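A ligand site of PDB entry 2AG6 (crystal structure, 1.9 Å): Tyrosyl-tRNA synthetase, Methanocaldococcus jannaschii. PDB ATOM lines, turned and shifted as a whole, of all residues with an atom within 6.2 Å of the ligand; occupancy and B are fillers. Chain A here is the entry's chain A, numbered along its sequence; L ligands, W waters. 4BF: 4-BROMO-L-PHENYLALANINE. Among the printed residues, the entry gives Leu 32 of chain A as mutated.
The side-chain amide oxygen (OE1) of Gln 173 sits at hydrogen-bond distance from a nitrogen (N) of the ligand. N of the ligand lies within hydrogen-bond range of OE1 of Gln 155, 2.8 Å away. OH of Tyr 151 lies within hydrogen-bond range of N of the ligand (2.9 Å). The backbone NH (N) of Glu 36 sits at hydrogen-bond distance from an oxygen (OXT) of the ligand (3.1 Å).
Water W3 bridges a ring nitrogen (NE2) of His 177 and the side-chain hydroxyl of Tyr 161.
Residues that only touch the ligand: Gly 34 (3.6 Å), Phe 35 (3.6 Å), Leu 65 (3.5 Å), Ala 67 (3.5 Å), His 70 (3.4 Å), His 160 (3.5 Å) and Tyr 161 (3.5 Å). Hydrophobic or aromatic side chains that line the ligand: Leu 65, Ala 67, His 70, Tyr 151 and His 160. 11 residues have an atom within 4 Å of the ligand: Gly 34, Phe 35, Glu 36, Leu 65, Ala 67, His 70, Tyr 151, Gln 155, His 160, Tyr 161 and Gln 173.
NE2 of His 70 is in hydrogen-bond range of N of Gln 155 (3.2 Å). The backbone carbonyl oxygen (O) of Gln 155 lies within hydrogen-bond range of the side-chain hydroxyl (OH) of Tyr 161, at 2.8 Å. A ring nitrogen (NE2) of His 177 sits at hydrogen-bond distance from the side-chain amide nitrogen (NE2) of Gln 155 (3.4 Å). OE2 of Glu 36 lies within hydrogen-bond range of OH of Tyr 151 (2.5 Å). OE2 of Glu 36 lies close to OD1 of Asn 74 (3.0 Å). The backbone NH of Ala 67 lies within hydrogen-bond range of the backbone carbonyl oxygen of Phe 35 (2.9 Å). The backbone carbonyl oxygen (O) of Met 154 sits at hydrogen-bond distance from a ring nitrogen (ND1) of His 160 (3.0 Å). The backbone carbonyl oxygen (O) of Leu 65 is in hydrogen-bond range of the backbone NH (N) of Phe 35 (3.0 Å).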
ATOM      1  N   LEU A  32       5.728   4.286   4.695  1.00  0.00           N
ATOM      2  CA  LEU A  32       6.143   5.655   4.542  1.00  0.00           C
ATOM      3  C   LEU A  32       6.821   6.185   5.804  1.00  0.00           C
ATOM      4  O   LEU A  32       6.421   5.864   6.908  1.00  0.00           O
ATOM      5  CB  LEU A  32       4.917   6.512   4.190  1.00  0.00           C
ATOM      6  CG  LEU A  32       5.042   8.038   4.371  1.00  0.00           C
ATOM      7  CD1 LEU A  32       5.672   8.533   3.132  1.00  0.00           C
ATOM      8  CD2 LEU A  32       3.672   8.721   4.607  1.00  0.00           C
ATOM      9  N   ILE A  33       7.850   6.998   5.629  1.00  0.00           N
ATOM     10  CA  ILE A  33       8.321   7.872   6.669  1.00  0.00           C
ATOM     11  C   ILE A  33       8.528   9.255   6.094  1.00  0.00           C
ATOM     12  O   ILE A  33       8.986   9.394   4.979  1.00  0.00           O
ATOM     13  CB  ILE A  33       9.590   7.360   7.413  1.00  0.00           C
ATOM     14  CG1 ILE A  33      10.002   8.309   8.540  1.00  0.00           C
ATOM     15  CG2 ILE A  33      10.757   7.158   6.457  1.00  0.00           C
ATOM     16  CD1 ILE A  33      10.926   7.617   9.596  1.00  0.00           C
ATOM     17  N   GLY A  34       8.165  10.275   6.849  1.00  0.00           N
ATOM     18  CA  GLY A  34       8.518  11.628   6.461  1.00  0.00           C
ATOM     19  C   GLY A  34       9.545  12.221   7.380  1.00  0.00           C
ATOM     20  O   GLY A  34       9.540  11.973   8.579  1.00  0.00           O
ATOM     21  N   PHE A  35      10.412  13.033   6.809  1.00  0.00           N
ATOM     22  CA  PHE A  35      11.391  13.803   7.567  1.00  0.00           C
ATOM     23  C   PHE A  35      11.334  15.232   7.108  1.00  0.00           C
ATOM     24  O   PHE A  35      11.429  15.475   5.940  1.00  0.00           O
ATOM     25  CB  PHE A  35      12.801  13.331   7.237  1.00  0.00           C
ATOM     26  CG  PHE A  35      13.121  11.953   7.671  1.00  0.00           C
ATOM     27  CD1 PHE A  35      13.205  10.935   6.752  1.00  0.00           C
ATOM     28  CD2 PHE A  35      13.347  11.673   9.001  1.00  0.00           C
ATOM     29  CE1 PHE A  35      13.533   9.659   7.146  1.00  0.00           C
ATOM     30  CE2 PHE A  35      13.680  10.374   9.393  1.00  0.00           C
ATOM     31  CZ  PHE A  35      13.741   9.385   8.476  1.00  0.00           C
ATOM     32  N   GLU A  36      11.245  16.191   8.022  1.00  0.00           N
ATOM     33  CA  GLU A  36      11.660  17.517   7.704  1.00  0.00           C
ATOM     34  C   GLU A  36      13.143  17.407   7.355  1.00  0.00           C
ATOM     35  O   GLU A  36      13.904  16.813   8.119  1.00  0.00           O
ATOM     36  CB  GLU A  36      11.509  18.432   8.920  1.00  0.00           C
ATOM     37  CG  GLU A  36      10.112  18.693   9.331  1.00  0.00           C
ATOM     38  CD  GLU A  36      10.068  19.643  10.484  1.00  0.00           C
ATOM     39  OE1 GLU A  36      10.872  20.589  10.470  1.00  0.00           O
ATOM     40  OE2 GLU A  36       9.238  19.457  11.392  1.00  0.00           O
ATOM     41  N   LEU A  65       9.142  10.566   2.386  1.00  0.00           N
ATOM     42  CA  LEU A  65       8.642  11.892   2.145  1.00  0.00           C
ATOM     43  C   LEU A  65       9.674  12.854   2.677  1.00  0.00           C
ATOM     44  O   LEU A  65      10.023  12.850   3.854  1.00  0.00           O
ATOM     45  CB  LEU A  65       7.328  12.071   2.865  1.00  0.00           C
ATOM     46  CG  LEU A  65       6.762  13.488   2.880  1.00  0.00           C
ATOM     47  CD1 LEU A  65       6.440  13.895   1.453  1.00  0.00           C
ATOM     48  CD2 LEU A  65       5.588  13.575   3.806  1.00  0.00           C
ATOM     49  N   ALA A  67       9.805  16.116   3.645  1.00  0.00           N
ATOM     50  CA  ALA A  67       8.662  16.931   4.099  1.00  0.00           C
ATOM     51  C   ALA A  67       9.053  18.394   4.065  1.00  0.00           C
ATOM     52  O   ALA A  67       9.195  19.034   5.090  1.00  0.00           O
ATOM     53  CB  ALA A  67       8.219  16.515   5.485  1.00  0.00           C
ATOM     54  N   HIS A  70       6.317  20.887   5.318  1.00  0.00           N
ATOM     55  CA  HIS A  70       6.267  20.811   6.795  1.00  0.00           C
ATOM     56  C   HIS A  70       7.400  21.519   7.474  1.00  0.00           C
ATOM     57  O   HIS A  70       7.208  22.288   8.420  1.00  0.00           O
ATOM     58  CB  HIS A  70       6.255  19.352   7.229  1.00  0.00           C
ATOM     59  CG  HIS A  70       4.902  18.754   7.202  1.00  0.00           C
ATOM     60  ND1 HIS A  70       4.383  18.188   6.064  1.00  0.00           N
ATOM     61  CD2 HIS A  70       3.939  18.664   8.156  1.00  0.00           C
ATOM     62  CE1 HIS A  70       3.163  17.738   6.330  1.00  0.00           C
ATOM     63  NE2 HIS A  70       2.874  18.008   7.591  1.00  0.00           N
ATOM     64  N   ASN A  74       7.458  24.684   9.850  1.00  0.00           N
ATOM     65  CA  ASN A  74       8.164  24.564  11.133  1.00  0.00           C
ATOM     66  C   ASN A  74       9.445  25.405  11.173  1.00  0.00           C
ATOM     67  O   ASN A  74      10.380  25.075  11.887  1.00  0.00           O
ATOM     68  CB  ASN A  74       8.483  23.110  11.429  1.00  0.00           C
ATOM     69  CG  ASN A  74       8.558  22.799  12.899  1.00  0.00           C
ATOM     70  OD1 ASN A  74       9.049  21.711  13.299  1.00  0.00           O
ATOM     71  ND2 ASN A  74       8.136  23.726  13.713  1.00  0.00           N
ATOM     72  N   GLN A 109       1.494  18.712  -2.099  1.00  0.00           N
ATOM     73  CA  GLN A 109       0.818  19.260  -0.950  1.00  0.00           C
ATOM     74  C   GLN A 109       0.158  20.595  -1.260  1.00  0.00           C
ATOM     75  O   GLN A 109      -0.508  21.150  -0.400  1.00  0.00           O
ATOM     76  CB  GLN A 109       1.776  19.406   0.204  1.00  0.00           C
ATOM     77  CG  GLN A 109       2.168  18.092   0.908  1.00  0.00           C
ATOM     78  CD  GLN A 109       3.060  18.389   2.100  1.00  0.00           C
ATOM     79  OE1 GLN A 109       2.602  18.500   3.250  1.00  0.00           O
ATOM     80  NE2 GLN A 109       4.293  18.647   1.818  1.00  0.00           N
ATOM     81  N   ILE A 137       7.589  18.681  18.607  1.00  0.00           N
ATOM     82  CA  ILE A 137       7.984  18.874  17.230  1.00  0.00           C
ATOM     83  C   ILE A 137       8.193  20.349  16.854  1.00  0.00           C
ATOM     84  O   ILE A 137       9.132  20.722  16.123  1.00  0.00           O
ATOM     85  CB  ILE A 137       6.893  18.237  16.339  1.00  0.00           C
ATOM     86  CG1 ILE A 137       6.913  16.724  16.547  1.00  0.00           C
ATOM     87  CG2 ILE A 137       7.085  18.548  14.895  1.00  0.00           C
ATOM     88  CD1 ILE A 137       5.612  16.047  16.182  1.00  0.00           C
ATOM     89  N   TYR A 151       0.611  22.423  10.547  1.00  0.00           N
ATOM     90  CA  TYR A 151       1.512  21.277  10.426  1.00  0.00           C
ATOM     91  C   TYR A 151       0.888  19.902  10.735  1.00  0.00           C
ATOM     92  O   TYR A 151       0.959  19.018   9.929  1.00  0.00           O
ATOM     93  CB  TYR A 151       2.722  21.599  11.268  1.00  0.00           C
ATOM     94  CG  TYR A 151       3.880  20.665  11.229  1.00  0.00           C
ATOM     95  CD1 TYR A 151       5.106  21.094  10.767  1.00  0.00           C
ATOM     96  CD2 TYR A 151       3.768  19.388  11.702  1.00  0.00           C
ATOM     97  CE1 TYR A 151       6.208  20.233  10.765  1.00  0.00           C
ATOM     98  CE2 TYR A 151       4.876  18.513  11.717  1.00  0.00           C
ATOM     99  CZ  TYR A 151       6.083  18.947  11.253  1.00  0.00           C
ATOM    100  OH  TYR A 151       7.167  18.102  11.270  1.00  0.00           O
ATOM    101  N   MET A 154      -1.832  18.859   8.241  1.00  0.00           N
ATOM    102  CA  MET A 154      -1.235  18.383   7.000  1.00  0.00           C
ATOM    103  C   MET A 154      -0.662  16.993   7.153  1.00  0.00           C
ATOM    104  O   MET A 154      -0.834  16.157   6.284  1.00  0.00           O
ATOM    105  CB  MET A 154      -0.104  19.287   6.553  1.00  0.00           C
ATOM    106  CG  MET A 154      -0.564  20.590   6.073  1.00  0.00           C
ATOM    107  SD  MET A 154       0.885  21.373   5.337  1.00  0.00           S
ATOM    108  CE  MET A 154       0.070  22.660   4.501  1.00  0.00           C
ATOM    109  N   GLN A 155      -0.013  16.736   8.279  1.00  0.00           N
ATOM    110  CA  GLN A 155       0.561  15.412   8.514  1.00  0.00           C
ATOM    111  C   GLN A 155      -0.508  14.291   8.569  1.00  0.00           C
ATOM    112  O   GLN A 155      -0.242  13.145   8.186  1.00  0.00           O
ATOM    113  CB  GLN A 155       1.491  15.418   9.714  1.00  0.00           C
ATOM    114  CG  GLN A 155       2.069  14.092  10.035  1.00  0.00           C
ATOM    115  CD  GLN A 155       3.273  14.199  10.914  1.00  0.00           C
ATOM    116  OE1 GLN A 155       3.842  15.235  11.052  1.00  0.00           O
ATOM    117  NE2 GLN A 155       3.677  13.064  11.508  1.00  0.00           N
ATOM    118  N   VAL A 156      -1.723  14.612   8.965  1.00  0.00           N
ATOM    119  CA  VAL A 156      -2.791  13.615   9.006  1.00  0.00           C
ATOM    120  C   VAL A 156      -3.620  13.577   7.734  1.00  0.00           C
ATOM    121  O   VAL A 156      -4.597  12.830   7.682  1.00  0.00           O
ATOM    122  CB  VAL A 156      -3.687  13.885  10.220  1.00  0.00           C
ATOM    123  CG1 VAL A 156      -4.937  13.094  10.222  1.00  0.00           C
ATOM    124  CG2 VAL A 156      -2.855  13.693  11.497  1.00  0.00           C
ATOM    125  N   HIS A 160      -1.500  11.755   2.081  1.00  0.00           N
ATOM    126  CA  HIS A 160      -0.183  11.235   2.375  1.00  0.00           C
ATOM    127  C   HIS A 160      -0.168   9.720   2.483  1.00  0.00           C
ATOM    128  O   HIS A 160       0.880   9.146   2.379  1.00  0.00           O
ATOM    129  CB  HIS A 160       0.303  11.760   3.699  1.00  0.00           C
ATOM    130  CG  HIS A 160       0.887  13.115   3.602  1.00  0.00           C
ATOM    131  ND1 HIS A 160       0.427  14.162   4.365  1.00  0.00           N
ATOM    132  CD2 HIS A 160       1.865  13.622   2.812  1.00  0.00           C
ATOM    133  CE1 HIS A 160       1.119  15.247   4.073  1.00  0.00           C
ATOM    134  NE2 HIS A 160       1.992  14.948   3.128  1.00  0.00           N
ATOM    135  N   TYR A 161      -1.303   9.079   2.761  1.00  0.00           N
ATOM    136  CA  TYR A 161      -1.313   7.688   3.119  1.00  0.00           C
ATOM    137  C   TYR A 161      -2.066   6.821   2.152  1.00  0.00           C
ATOM    138  O   TYR A 161      -2.305   5.691   2.461  1.00  0.00           O
ATOM    139  CB  TYR A 161      -1.917   7.493   4.507  1.00  0.00           C
ATOM    140  CG  TYR A 161      -1.192   8.305   5.541  1.00  0.00           C
ATOM    141  CD1 TYR A 161      -1.706   9.505   5.975  1.00  0.00           C
ATOM    142  CD2 TYR A 161       0.054   7.915   6.005  1.00  0.00           C
ATOM    143  CE1 TYR A 161      -1.003  10.289   6.899  1.00  0.00           C
ATOM    144  CE2 TYR A 161       0.729   8.667   6.912  1.00  0.00           C
ATOM    145  CZ  TYR A 161       0.198   9.847   7.378  1.00  0.00           C
ATOM    146  OH  TYR A 161       0.910  10.613   8.254  1.00  0.00           O
ATOM    147  N   GLU A 172       8.069  10.964  19.069  1.00  0.00           N
ATOM    148  CA  GLU A 172       7.636  12.375  19.087  1.00  0.00           C
ATOM    149  C   GLU A 172       6.446  12.607  18.221  1.00  0.00           C
ATOM    150  O   GLU A 172       5.713  13.579  18.411  1.00  0.00           O
ATOM    151  CB  GLU A 172       8.657  13.403  18.588  1.00  0.00           C
ATOM    152  CG  GLU A 172      10.083  13.064  18.550  1.00  0.00           C
ATOM    153  CD  GLU A 172      10.365  12.151  17.380  1.00  0.00           C
ATOM    154  OE1 GLU A 172      10.229  12.534  16.190  1.00  0.00           O
ATOM    155  OE2 GLU A 172      10.685  11.018  17.684  1.00  0.00           O
ATOM    156  N   GLN A 173       6.273  11.768  17.202  1.00  0.00           N
ATOM    157  CA  GLN A 173       5.154  11.868  16.324  1.00  0.00           C
ATOM    158  C   GLN A 173       3.871  11.281  16.863  1.00  0.00           C
ATOM    159  O   GLN A 173       2.862  11.329  16.162  1.00  0.00           O
ATOM    160  CB  GLN A 173       5.437  11.157  14.996  1.00  0.00           C
ATOM    161  CG  GLN A 173       6.763  11.478  14.310  1.00  0.00           C
ATOM    162  CD  GLN A 173       6.952  12.933  14.001  1.00  0.00           C
ATOM    163  OE1 GLN A 173       6.058  13.587  13.469  1.00  0.00           O
ATOM    164  NE2 GLN A 173       8.144  13.463  14.339  1.00  0.00           N
ATOM    165  N   ILE A 176       0.458  13.270  16.957  1.00  0.00           N
ATOM    166  CA  ILE A 176      -0.020  13.494  15.602  1.00  0.00           C
ATOM    167  C   ILE A 176      -0.588  12.202  15.043  1.00  0.00           C
ATOM    168  O   ILE A 176      -1.634  12.178  14.469  1.00  0.00           O
ATOM    169  CB  ILE A 176       1.047  13.995  14.694  1.00  0.00           C
ATOM    170  CG1 ILE A 176       1.465  15.389  15.089  1.00  0.00           C
ATOM    171  CG2 ILE A 176       0.579  14.044  13.284  1.00  0.00           C
ATOM    172  CD1 ILE A 176       2.557  15.972  14.267  1.00  0.00           C
ATOM    173  N   HIS A 177       0.135  11.112  15.189  1.00  0.00           N
ATOM    174  CA  HIS A 177      -0.360   9.858  14.625  1.00  0.00           C
ATOM    175  C   HIS A 177      -1.637   9.400  15.278  1.00  0.00           C
ATOM    176  O   HIS A 177      -2.458   8.826  14.617  1.00  0.00           O
ATOM    177  CB  HIS A 177       0.710   8.803  14.656  1.00  0.00           C
ATOM    178  CG  HIS A 177       1.792   9.064  13.675  1.00  0.00           C
ATOM    179  ND1 HIS A 177       2.999   8.421  13.723  1.00  0.00           N
ATOM    180  CD2 HIS A 177       1.872   9.920  12.636  1.00  0.00           C
ATOM    181  CE1 HIS A 177       3.773   8.856  12.749  1.00  0.00           C
ATOM    182  NE2 HIS A 177       3.109   9.763  12.061  1.00  0.00           N
HETATM  183  CD1 4BF L   1       6.185  13.213   8.769  1.00  0.00           C
HETATM  184  CE1 4BF L   1       5.141  12.654   8.102  1.00  0.00           C
HETATM  185  CZ  4BF L   1       4.443  13.465   7.230  1.00  0.00           C
HETATM  186 BR   4BF L   1       2.999  12.748   6.360  1.00  0.00          BR
HETATM  187  CE2 4BF L   1       4.724  14.778   7.019  1.00  0.00           C
HETATM  188  CD2 4BF L   1       5.816  15.325   7.689  1.00  0.00           C
HETATM  189  CG  4BF L   1       6.529  14.533   8.566  1.00  0.00           C
HETATM  190  CB  4BF L   1       7.709  15.113   9.304  1.00  0.00           C
HETATM  191  CA  4BF L   1       7.777  14.772  10.765  1.00  0.00           C
HETATM  192  N   4BF L   1       6.566  15.259  11.448  1.00  0.00           N
HETATM  193  C   4BF L   1       8.946  15.512  11.338  1.00  0.00           C
HETATM  194  OXT 4BF L   1      10.143  15.099  10.678  1.00  0.00           O
HETATM  195  O   4BF L   1       9.081  15.607  12.545  1.00  0.00           O
HETATM  196  O   HOH W   1      10.737  17.183  13.741  1.00  0.00           O
HETATM  197  O   HOH W   2       8.246  11.225  10.769  1.00  0.00           O
HETATM  198  O   HOH W   3       3.533   9.894   9.317  1.00  0.00           O
HETATM  199  O   HOH W   4      12.403  14.454  11.420  1.00  0.00           O
